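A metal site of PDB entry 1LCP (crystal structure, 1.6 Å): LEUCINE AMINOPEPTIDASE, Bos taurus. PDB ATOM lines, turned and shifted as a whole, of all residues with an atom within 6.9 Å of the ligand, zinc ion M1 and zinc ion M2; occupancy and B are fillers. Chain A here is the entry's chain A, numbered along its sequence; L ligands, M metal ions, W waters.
The side-chain carboxylate (OD2) of Asp 255 sits close to the side-chain amino group (NZ) of Lys 262 (3.7 Å).
The side-chain amino group (NZ) of Lys 262 lies within salt-bridge range of the side-chain carboxylate (OD2) of Asp 332, 2.9 Å away.
N of Gly 257 is in hydrogen-bond range of OD1 of Asp 255, at 3.0 Å.
The side-chain carboxylate (OD1) of Asp 255 sits close to the side-chain amide oxygen (OD1) of Asn 305 (3.0 Å).
N of Ile 252 sits at hydrogen-bond distance from O of Asp 273, 3.3 Å away.
OD1 of Asp 273 is in hydrogen-bond range of OG1 of Thr 359 (2.7 Å).
The backbone NH (N) of Ala 451 sits at hydrogen-bond distance from the side-chain carboxylate (OD1) of Asp 449 (3.3 Å).
OD1 of Asn 305 sits close to OE1 of Glu 334 (3.4 Å).
Four residues have an atom within 4 Å of zinc ion M2: Lys 250, Asp 255, Asp 273 and Glu 334.
The backbone carbonyl oxygen (O) of Leu 360 lies close to an oxygen (O3) of the ligand, at 3.2 Å.
Merely in contact with the ligand: Thr 359 (3.6 Å), Ala 451 (3.7 Å) and Met 270 (3.8 Å).
Hydrophobic or aromatic side chains within 4 Å of the ligand: Met 270 and Ala 451.
Of the 29 residues printed, 10 come within 4 Å of the ligand.
The nearest printed residue that does not touch the ligand is Gly 335 (4.3 Å).
Merely in contact with zinc ion M1: Lys 262 (3.7 Å).
Of the 29 residues printed, 4 come within 4 Å of zinc ion M1.
Water W1 lies within hydrogen-bond range of an oxygen (O3) of the ligand and the backbone NH of Gly 362.
Water W2 lies within hydrogen-bond range of O3 of the ligand (2.8 Å), NH2 of Arg 336 (2.8 Å) and O of Leu 360 (3.2 Å).
Zinc ion M2 is bound by the side-chain carboxylate (OE2) of Glu 334 (2.1 Å), the side-chain carboxylate (OD2) of Asp 273 (2.1 Å), the side-chain amino group (NZ) of Lys 250 (2.1 Å), an oxygen (O1) of the ligand (2.3 Å) and a nitrogen (N1) of the ligand (2.3 Å).
Zinc ion M2 has five donor atoms within binding distance.
Slightly farther from zinc ion M2 lies OD2 of Asp 255 (2.7 Å).
Zinc ion M1 is bound by the side-chain carboxylate of Glu 334 (2.0 Å), the side-chain carboxylate of Asp 332 (2.0 Å), an oxygen (O2) of the ligand (2.1 Å), the side-chain carboxylate of Asp 255 (2.1 Å), the backbone carbonyl oxygen of Asp 332 (2.2 Å) and an oxygen (O1) of the ligand (2.5 Å).
Zinc ion M1 has six donor atoms within binding distance.
An oxygen (O2) of the ligand lies close to the side-chain amino group (NZ) of Lys 262 (2.7 Å).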
ATOM      1  N   LYS A 250       4.172 -25.952  -6.260  1.00  0.00           N
ATOM      2  CA  LYS A 250       5.565 -25.548  -5.953  1.00  0.00           C
ATOM      3  C   LYS A 250       5.911 -25.965  -4.501  1.00  0.00           C
ATOM      4  O   LYS A 250       5.256 -25.526  -3.549  1.00  0.00           O
ATOM      5  CB  LYS A 250       5.713 -24.022  -6.100  1.00  0.00           C
ATOM      6  CG  LYS A 250       7.068 -23.458  -5.660  1.00  0.00           C
ATOM      7  CD  LYS A 250       7.086 -21.918  -5.663  1.00  0.00           C
ATOM      8  CE  LYS A 250       8.364 -21.342  -5.015  1.00  0.00           C
ATOM      9  NZ  LYS A 250       8.385 -19.833  -4.999  1.00  0.00           N
ATOM     10  N   ILE A 252       8.939 -25.550  -2.477  1.00  0.00           N
ATOM     11  CA  ILE A 252      10.229 -25.068  -1.932  1.00  0.00           C
ATOM     12  C   ILE A 252      10.050 -25.028  -0.399  1.00  0.00           C
ATOM     13  O   ILE A 252       9.366 -24.147   0.122  1.00  0.00           O
ATOM     14  CB  ILE A 252      10.608 -23.676  -2.476  1.00  0.00           C
ATOM     15  CG1 ILE A 252      10.846 -23.705  -3.994  1.00  0.00           C
ATOM     16  CG2 ILE A 252      11.844 -23.144  -1.752  1.00  0.00           C
ATOM     17  CD1 ILE A 252      12.060 -24.530  -4.426  1.00  0.00           C
ATOM     18  N   ASP A 255      13.056 -21.049   1.169  1.00  0.00           N
ATOM     19  CA  ASP A 255      13.652 -20.222   0.117  1.00  0.00           C
ATOM     20  C   ASP A 255      14.525 -19.110   0.699  1.00  0.00           C
ATOM     21  O   ASP A 255      14.004 -18.099   1.194  1.00  0.00           O
ATOM     22  CB  ASP A 255      12.541 -19.604  -0.740  1.00  0.00           C
ATOM     23  CG  ASP A 255      13.075 -18.889  -1.995  1.00  0.00           C
ATOM     24  OD1 ASP A 255      14.285 -19.024  -2.328  1.00  0.00           O
ATOM     25  OD2 ASP A 255      12.270 -18.192  -2.648  1.00  0.00           O
ATOM     26  N   SER A 256      15.843 -19.295   0.624  1.00  0.00           N
ATOM     27  CA  SER A 256      16.801 -18.295   1.109  1.00  0.00           C
ATOM     28  C   SER A 256      17.181 -17.366  -0.055  1.00  0.00           C
ATOM     29  O   SER A 256      17.868 -16.361   0.163  1.00  0.00           O
ATOM     30  CB  SER A 256      18.078 -18.973   1.604  1.00  0.00           C
ATOM     31  OG  SER A 256      18.909 -19.367   0.513  1.00  0.00           O
ATOM     32  N   GLY A 257      16.804 -17.745  -1.273  1.00  0.00           N
ATOM     33  CA  GLY A 257      17.159 -16.984  -2.455  1.00  0.00           C
ATOM     34  C   GLY A 257      18.394 -17.555  -3.155  1.00  0.00           C
ATOM     35  O   GLY A 257      18.582 -17.360  -4.363  1.00  0.00           O
ATOM     36  N   GLY A 258      19.212 -18.287  -2.402  1.00  0.00           N
ATOM     37  CA  GLY A 258      20.430 -18.870  -2.957  1.00  0.00           C
ATOM     38  C   GLY A 258      21.520 -17.813  -3.076  1.00  0.00           C
ATOM     39  O   GLY A 258      21.631 -16.943  -2.210  1.00  0.00           O
ATOM     40  N   SER A 260      21.615 -15.369  -5.095  1.00  0.00           N
ATOM     41  CA  SER A 260      20.891 -14.097  -5.191  1.00  0.00           C
ATOM     42  C   SER A 260      20.099 -14.041  -3.849  1.00  0.00           C
ATOM     43  O   SER A 260      18.856 -14.055  -3.830  1.00  0.00           O
ATOM     44  CB  SER A 260      19.927 -14.128  -6.387  1.00  0.00           C
ATOM     45  OG  SER A 260      20.593 -14.383  -7.630  1.00  0.00           O
ATOM     46  N   LYS A 262      18.240 -13.443  -0.244  1.00  0.00           N
ATOM     47  CA  LYS A 262      17.178 -12.555   0.237  1.00  0.00           C
ATOM     48  C   LYS A 262      17.671 -11.704   1.393  1.00  0.00           C
ATOM     49  O   LYS A 262      18.690 -12.022   2.016  1.00  0.00           O
ATOM     50  CB  LYS A 262      15.997 -13.378   0.747  1.00  0.00           C
ATOM     51  CG  LYS A 262      15.177 -14.064  -0.331  1.00  0.00           C
ATOM     52  CD  LYS A 262      13.955 -14.749   0.286  1.00  0.00           C
ATOM     53  CE  LYS A 262      13.125 -15.480  -0.758  1.00  0.00           C
ATOM     54  NZ  LYS A 262      12.643 -14.580  -1.842  1.00  0.00           N
ATOM     55  N   MET A 270       9.476 -17.683   4.622  1.00  0.00           N
ATOM     56  CA  MET A 270       9.807 -18.505   3.468  1.00  0.00           C
ATOM     57  C   MET A 270       9.736 -20.012   3.759  1.00  0.00           C
ATOM     58  O   MET A 270       9.940 -20.827   2.847  1.00  0.00           O
ATOM     59  CB  MET A 270      11.162 -18.070   2.856  1.00  0.00           C
ATOM     60  CG  MET A 270      11.140 -16.637   2.246  1.00  0.00           C
ATOM     61  SD  MET A 270       9.869 -16.428   0.925  1.00  0.00           S
ATOM     62  CE  MET A 270       8.595 -15.589   1.802  1.00  0.00           C
ATOM     63  N   ASP A 273       7.125 -21.454   1.554  1.00  0.00           N
ATOM     64  CA  ASP A 273       7.295 -21.399   0.093  1.00  0.00           C
ATOM     65  C   ASP A 273       6.903 -22.719  -0.593  1.00  0.00           C
ATOM     66  O   ASP A 273       7.109 -22.908  -1.793  1.00  0.00           O
ATOM     67  CB  ASP A 273       8.719 -20.975  -0.283  1.00  0.00           C
ATOM     68  CG  ASP A 273       8.779 -20.246  -1.627  1.00  0.00           C
ATOM     69  OD1 ASP A 273       7.769 -19.612  -2.036  1.00  0.00           O
ATOM     70  OD2 ASP A 273       9.841 -20.315  -2.267  1.00  0.00           O
ATOM     71  N   ASN A 305      16.142 -24.025  -1.347  1.00  0.00           N
ATOM     72  CA  ASN A 305      16.916 -23.121  -2.216  1.00  0.00           C
ATOM     73  C   ASN A 305      17.914 -22.451  -1.260  1.00  0.00           C
ATOM     74  O   ASN A 305      17.571 -21.510  -0.546  1.00  0.00           O
ATOM     75  CB  ASN A 305      15.990 -22.085  -2.894  1.00  0.00           C
ATOM     76  CG  ASN A 305      16.724 -21.231  -3.938  1.00  0.00           C
ATOM     77  OD1 ASN A 305      16.328 -20.085  -4.194  1.00  0.00           O
ATOM     78  ND2 ASN A 305      17.748 -21.777  -4.550  1.00  0.00           N
ATOM     79  N   ASN A 330      18.624 -14.807 -12.035  1.00  0.00           N
ATOM     80  CA  ASN A 330      18.412 -14.548 -10.600  1.00  0.00           C
ATOM     81  C   ASN A 330      18.032 -15.896  -9.963  1.00  0.00           C
ATOM     82  O   ASN A 330      16.970 -16.449 -10.245  1.00  0.00           O
ATOM     83  CB  ASN A 330      17.295 -13.519 -10.409  1.00  0.00           C
ATOM     84  CG  ASN A 330      17.174 -13.028  -8.975  1.00  0.00           C
ATOM     85  OD1 ASN A 330      17.279 -11.820  -8.685  1.00  0.00           O
ATOM     86  ND2 ASN A 330      16.933 -13.950  -8.068  1.00  0.00           N
ATOM     87  N   THR A 331      18.900 -16.395  -9.075  1.00  0.00           N
ATOM     88  CA  THR A 331      18.676 -17.700  -8.433  1.00  0.00           C
ATOM     89  C   THR A 331      17.462 -17.748  -7.500  1.00  0.00           C
ATOM     90  O   THR A 331      16.999 -18.826  -7.119  1.00  0.00           O
ATOM     91  CB  THR A 331      19.947 -18.192  -7.669  1.00  0.00           C
ATOM     92  OG1 THR A 331      20.195 -17.361  -6.520  1.00  0.00           O
ATOM     93  CG2 THR A 331      21.199 -18.129  -8.595  1.00  0.00           C
ATOM     94  N   ASP A 332      16.957 -16.567  -7.121  1.00  0.00           N
ATOM     95  CA  ASP A 332      15.789 -16.442  -6.247  1.00  0.00           C
ATOM     96  C   ASP A 332      14.456 -16.544  -7.018  1.00  0.00           C
ATOM     97  O   ASP A 332      13.369 -16.454  -6.441  1.00  0.00           O
ATOM     98  CB  ASP A 332      15.888 -15.145  -5.436  1.00  0.00           C
ATOM     99  CG  ASP A 332      14.938 -15.106  -4.239  1.00  0.00           C
ATOM    100  OD1 ASP A 332      14.426 -16.156  -3.799  1.00  0.00           O
ATOM    101  OD2 ASP A 332      14.727 -13.988  -3.722  1.00  0.00           O
ATOM    102  N   ALA A 333      14.519 -16.638  -8.333  1.00  0.00           N
ATOM    103  CA  ALA A 333      13.309 -16.814  -9.137  1.00  0.00           C
ATOM    104  C   ALA A 333      13.325 -18.329  -9.378  1.00  0.00           C
ATOM    105  O   ALA A 333      13.298 -18.808 -10.524  1.00  0.00           O
ATOM    106  CB  ALA A 333      13.398 -16.042 -10.452  1.00  0.00           C
ATOM    107  N   GLU A 334      13.357 -19.087  -8.283  1.00  0.00           N
ATOM    108  CA  GLU A 334      13.459 -20.535  -8.360  1.00  0.00           C
ATOM    109  C   GLU A 334      12.170 -21.312  -8.556  1.00  0.00           C
ATOM    110  O   GLU A 334      12.212 -22.466  -9.029  1.00  0.00           O
ATOM    111  CB  GLU A 334      14.213 -21.062  -7.130  1.00  0.00           C
ATOM    112  CG  GLU A 334      13.377 -21.331  -5.866  1.00  0.00           C
ATOM    113  CD  GLU A 334      12.711 -20.092  -5.286  1.00  0.00           C
ATOM    114  OE1 GLU A 334      13.331 -19.012  -5.306  1.00  0.00           O
ATOM    115  OE2 GLU A 334      11.577 -20.222  -4.787  1.00  0.00           O
ATOM    116  N   GLY A 335      11.044 -20.733  -8.147  1.00  0.00           N
ATOM    117  CA  GLY A 335       9.762 -21.421  -8.275  1.00  0.00           C
ATOM    118  C   GLY A 335       9.441 -21.767  -9.716  1.00  0.00           C
ATOM    119  O   GLY A 335       9.035 -22.900 -10.016  1.00  0.00           O
ATOM    120  N   ARG A 336       9.663 -20.831 -10.619  1.00  0.00           N
ATOM    121  CA  ARG A 336       9.375 -21.091 -12.025  1.00  0.00           C
ATOM    122  C   ARG A 336      10.315 -22.151 -12.610  1.00  0.00           C
ATOM    123  O   ARG A 336       9.927 -22.895 -13.524  1.00  0.00           O
ATOM    124  CB  ARG A 336       9.400 -19.786 -12.838  1.00  0.00           C
ATOM    125  CG  ARG A 336      10.730 -19.134 -13.010  1.00  0.00           C
ATOM    126  CD  ARG A 336      10.540 -17.702 -13.507  1.00  0.00           C
ATOM    127  NE  ARG A 336      10.135 -16.812 -12.420  1.00  0.00           N
ATOM    128  CZ  ARG A 336       9.834 -15.524 -12.565  1.00  0.00           C
ATOM    129  NH1 ARG A 336       9.841 -14.935 -13.761  1.00  0.00           N
ATOM    130  NH2 ARG A 336       9.503 -14.811 -11.500  1.00  0.00           N
ATOM    131  N   THR A 359       3.406 -20.098  -4.501  1.00  0.00           N
ATOM    132  CA  THR A 359       3.646 -18.840  -3.788  1.00  0.00           C
ATOM    133  C   THR A 359       4.743 -18.281  -4.713  1.00  0.00           C
ATOM    134  O   THR A 359       5.912 -18.196  -4.352  1.00  0.00           O
ATOM    135  CB  THR A 359       4.206 -19.142  -2.363  1.00  0.00           C
ATOM    136  OG1 THR A 359       5.186 -20.194  -2.440  1.00  0.00           O
ATOM    137  CG2 THR A 359       3.069 -19.608  -1.423  1.00  0.00           C
ATOM    138  N   LEU A 360       4.350 -17.926  -5.941  1.00  0.00           N
ATOM    139  CA  LEU A 360       5.306 -17.525  -6.966  1.00  0.00           C
ATOM    140  C   LEU A 360       6.008 -16.174  -6.974  1.00  0.00           C
ATOM    141  O   LEU A 360       7.223 -16.113  -7.218  1.00  0.00           O
ATOM    142  CB  LEU A 360       4.718 -17.803  -8.359  1.00  0.00           C
ATOM    143  CG  LEU A 360       5.747 -18.035  -9.478  1.00  0.00           C
ATOM    144  CD1 LEU A 360       6.507 -19.341  -9.207  1.00  0.00           C
ATOM    145  CD2 LEU A 360       5.076 -18.108 -10.850  1.00  0.00           C
ATOM    146  N   THR A 361       5.283 -15.082  -6.753  1.00  0.00           N
ATOM    147  CA  THR A 361       5.926 -13.775  -6.825  1.00  0.00           C
ATOM    148  C   THR A 361       5.533 -12.744  -5.772  1.00  0.00           C
ATOM    149  O   THR A 361       4.378 -12.663  -5.366  1.00  0.00           O
ATOM    150  CB  THR A 361       5.636 -13.125  -8.227  1.00  0.00           C
ATOM    151  OG1 THR A 361       4.230 -12.839  -8.341  1.00  0.00           O
ATOM    152  CG2 THR A 361       6.093 -14.031  -9.391  1.00  0.00           C
ATOM    153  N   GLY A 362       6.500 -11.934  -5.359  1.00  0.00           N
ATOM    154  CA  GLY A 362       6.184 -10.870  -4.422  1.00  0.00           C
ATOM    155  C   GLY A 362       5.284  -9.881  -5.170  1.00  0.00           C
ATOM    156  O   GLY A 362       4.440  -9.210  -4.567  1.00  0.00           O
ATOM    157  N   ALA A 363       5.453  -9.812  -6.488  1.00  0.00           N
ATOM    158  CA  ALA A 363       4.655  -8.917  -7.335  1.00  0.00           C
ATOM    159  C   ALA A 363       3.152  -9.175  -7.192  1.00  0.00           C
ATOM    160  O   ALA A 363       2.356  -8.232  -7.203  1.00  0.00           O
ATOM    161  CB  ALA A 363       5.079  -9.051  -8.798  1.00  0.00           C
ATOM    162  N   ASP A 365       1.691 -10.174  -4.538  1.00  0.00           N
ATOM    163  CA  ASP A 365       1.291  -9.573  -3.264  1.00  0.00           C
ATOM    164  C   ASP A 365       1.109  -8.053  -3.420  1.00  0.00           C
ATOM    165  O   ASP A 365       0.165  -7.462  -2.889  1.00  0.00           O
ATOM    166  CB  ASP A 365       2.320  -9.873  -2.176  1.00  0.00           C
ATOM    167  CG  ASP A 365       1.896  -9.298  -0.827  1.00  0.00           C
ATOM    168  OD1 ASP A 365       0.828  -9.691  -0.319  1.00  0.00           O
ATOM    169  OD2 ASP A 365       2.594  -8.418  -0.313  1.00  0.00           O
ATOM    170  N   ASP A 449      -1.334 -18.003  -8.547  1.00  0.00           N
ATOM    171  CA  ASP A 449      -0.223 -17.408  -7.803  1.00  0.00           C
ATOM    172  C   ASP A 449      -0.846 -17.039  -6.441  1.00  0.00           C
ATOM    173  O   ASP A 449      -1.637 -16.091  -6.341  1.00  0.00           O
ATOM    174  CB  ASP A 449       0.331 -16.151  -8.518  1.00  0.00           C
ATOM    175  CG  ASP A 449       1.650 -15.647  -7.904  1.00  0.00           C
ATOM    176  OD1 ASP A 449       1.949 -15.940  -6.720  1.00  0.00           O
ATOM    177  OD2 ASP A 449       2.410 -14.954  -8.629  1.00  0.00           O
ATOM    178  N   ILE A 450      -0.495 -17.817  -5.421  1.00  0.00           N
ATOM    179  CA  ILE A 450      -1.025 -17.638  -4.064  1.00  0.00           C
ATOM    180  C   ILE A 450      -0.097 -16.898  -3.086  1.00  0.00           C
ATOM    181  O   ILE A 450      -0.348 -16.882  -1.881  1.00  0.00           O
ATOM    182  CB  ILE A 450      -1.420 -19.013  -3.448  1.00  0.00           C
ATOM    183  CG1 ILE A 450      -0.179 -19.903  -3.265  1.00  0.00           C
ATOM    184  CG2 ILE A 450      -2.464 -19.717  -4.329  1.00  0.00           C
ATOM    185  CD1 ILE A 450      -0.409 -21.107  -2.363  1.00  0.00           C
ATOM    186  N   ALA A 451       0.948 -16.259  -3.609  1.00  0.00           N
ATOM    187  CA  ALA A 451       1.890 -15.528  -2.757  1.00  0.00           C
ATOM    188  C   ALA A 451       1.217 -14.514  -1.836  1.00  0.00           C
ATOM    189  O   ALA A 451       1.569 -14.398  -0.659  1.00  0.00           O
ATOM    190  CB  ALA A 451       2.936 -14.837  -3.624  1.00  0.00           C
ATOM    191  N   GLY A 452       0.226 -13.791  -2.358  1.00  0.00           N
ATOM    192  CA  GLY A 452      -0.486 -12.794  -1.563  1.00  0.00           C
ATOM    193  C   GLY A 452      -1.394 -13.325  -0.468  1.00  0.00           C
ATOM    194  O   GLY A 452      -1.683 -12.611   0.506  1.00  0.00           O
ATOM    195  N   MET A 454      -0.660 -16.148   1.280  1.00  0.00           N
ATOM    196  CA  MET A 454       0.145 -17.075   2.060  1.00  0.00           C
ATOM    197  C   MET A 454      -0.168 -16.954   3.568  1.00  0.00           C
ATOM    198  O   MET A 454      -0.267 -17.960   4.285  1.00  0.00           O
ATOM    199  CB  MET A 454       1.639 -16.801   1.849  1.00  0.00           C
ATOM    200  CG  MET A 454       2.557 -17.620   2.777  1.00  0.00           C
ATOM    201  SD  MET A 454       4.350 -17.393   2.534  1.00  0.00           S
ATOM    202  CE  MET A 454       4.634 -15.974   3.524  1.00  0.00           C
HETATM  203  C1  LIG L   1       8.957 -16.180  -3.754  1.00  0.00           C
HETATM  204  C2  LIG L   1       8.781 -14.873  -2.982  1.00  0.00           C
HETATM  205  C3  LIG L   1       7.704 -14.847  -1.852  1.00  0.00           C
HETATM  206  C4  LIG L   1       6.323 -15.273  -2.319  1.00  0.00           C
HETATM  207  C5  LIG L   1       7.613 -13.471  -1.167  1.00  0.00           C
HETATM  208  N1  LIG L   1       9.265 -17.261  -2.808  1.00  0.00           N
HETATM  209  P1  LIG L   1      10.361 -16.041  -4.892  1.00  0.00           P
HETATM  210  O1  LIG L   1      10.600 -17.458  -5.464  1.00  0.00           O
HETATM  211  O2  LIG L   1      11.642 -15.567  -4.122  1.00  0.00           O
HETATM  212  O3  LIG L   1       9.998 -15.016  -5.977  1.00  0.00           O
HETATM  213 ZN    ZN M   1      12.862 -17.253  -4.453  1.00  0.00          ZN
HETATM  214 ZN    ZN M   2      10.072 -19.062  -3.959  1.00  0.00          ZN
HETATM  215  O   HOH W   1       9.256 -12.536  -5.791  1.00  0.00           O
HETATM  216  O   HOH W   2       9.932 -15.284  -8.731  1.00  0.00           O
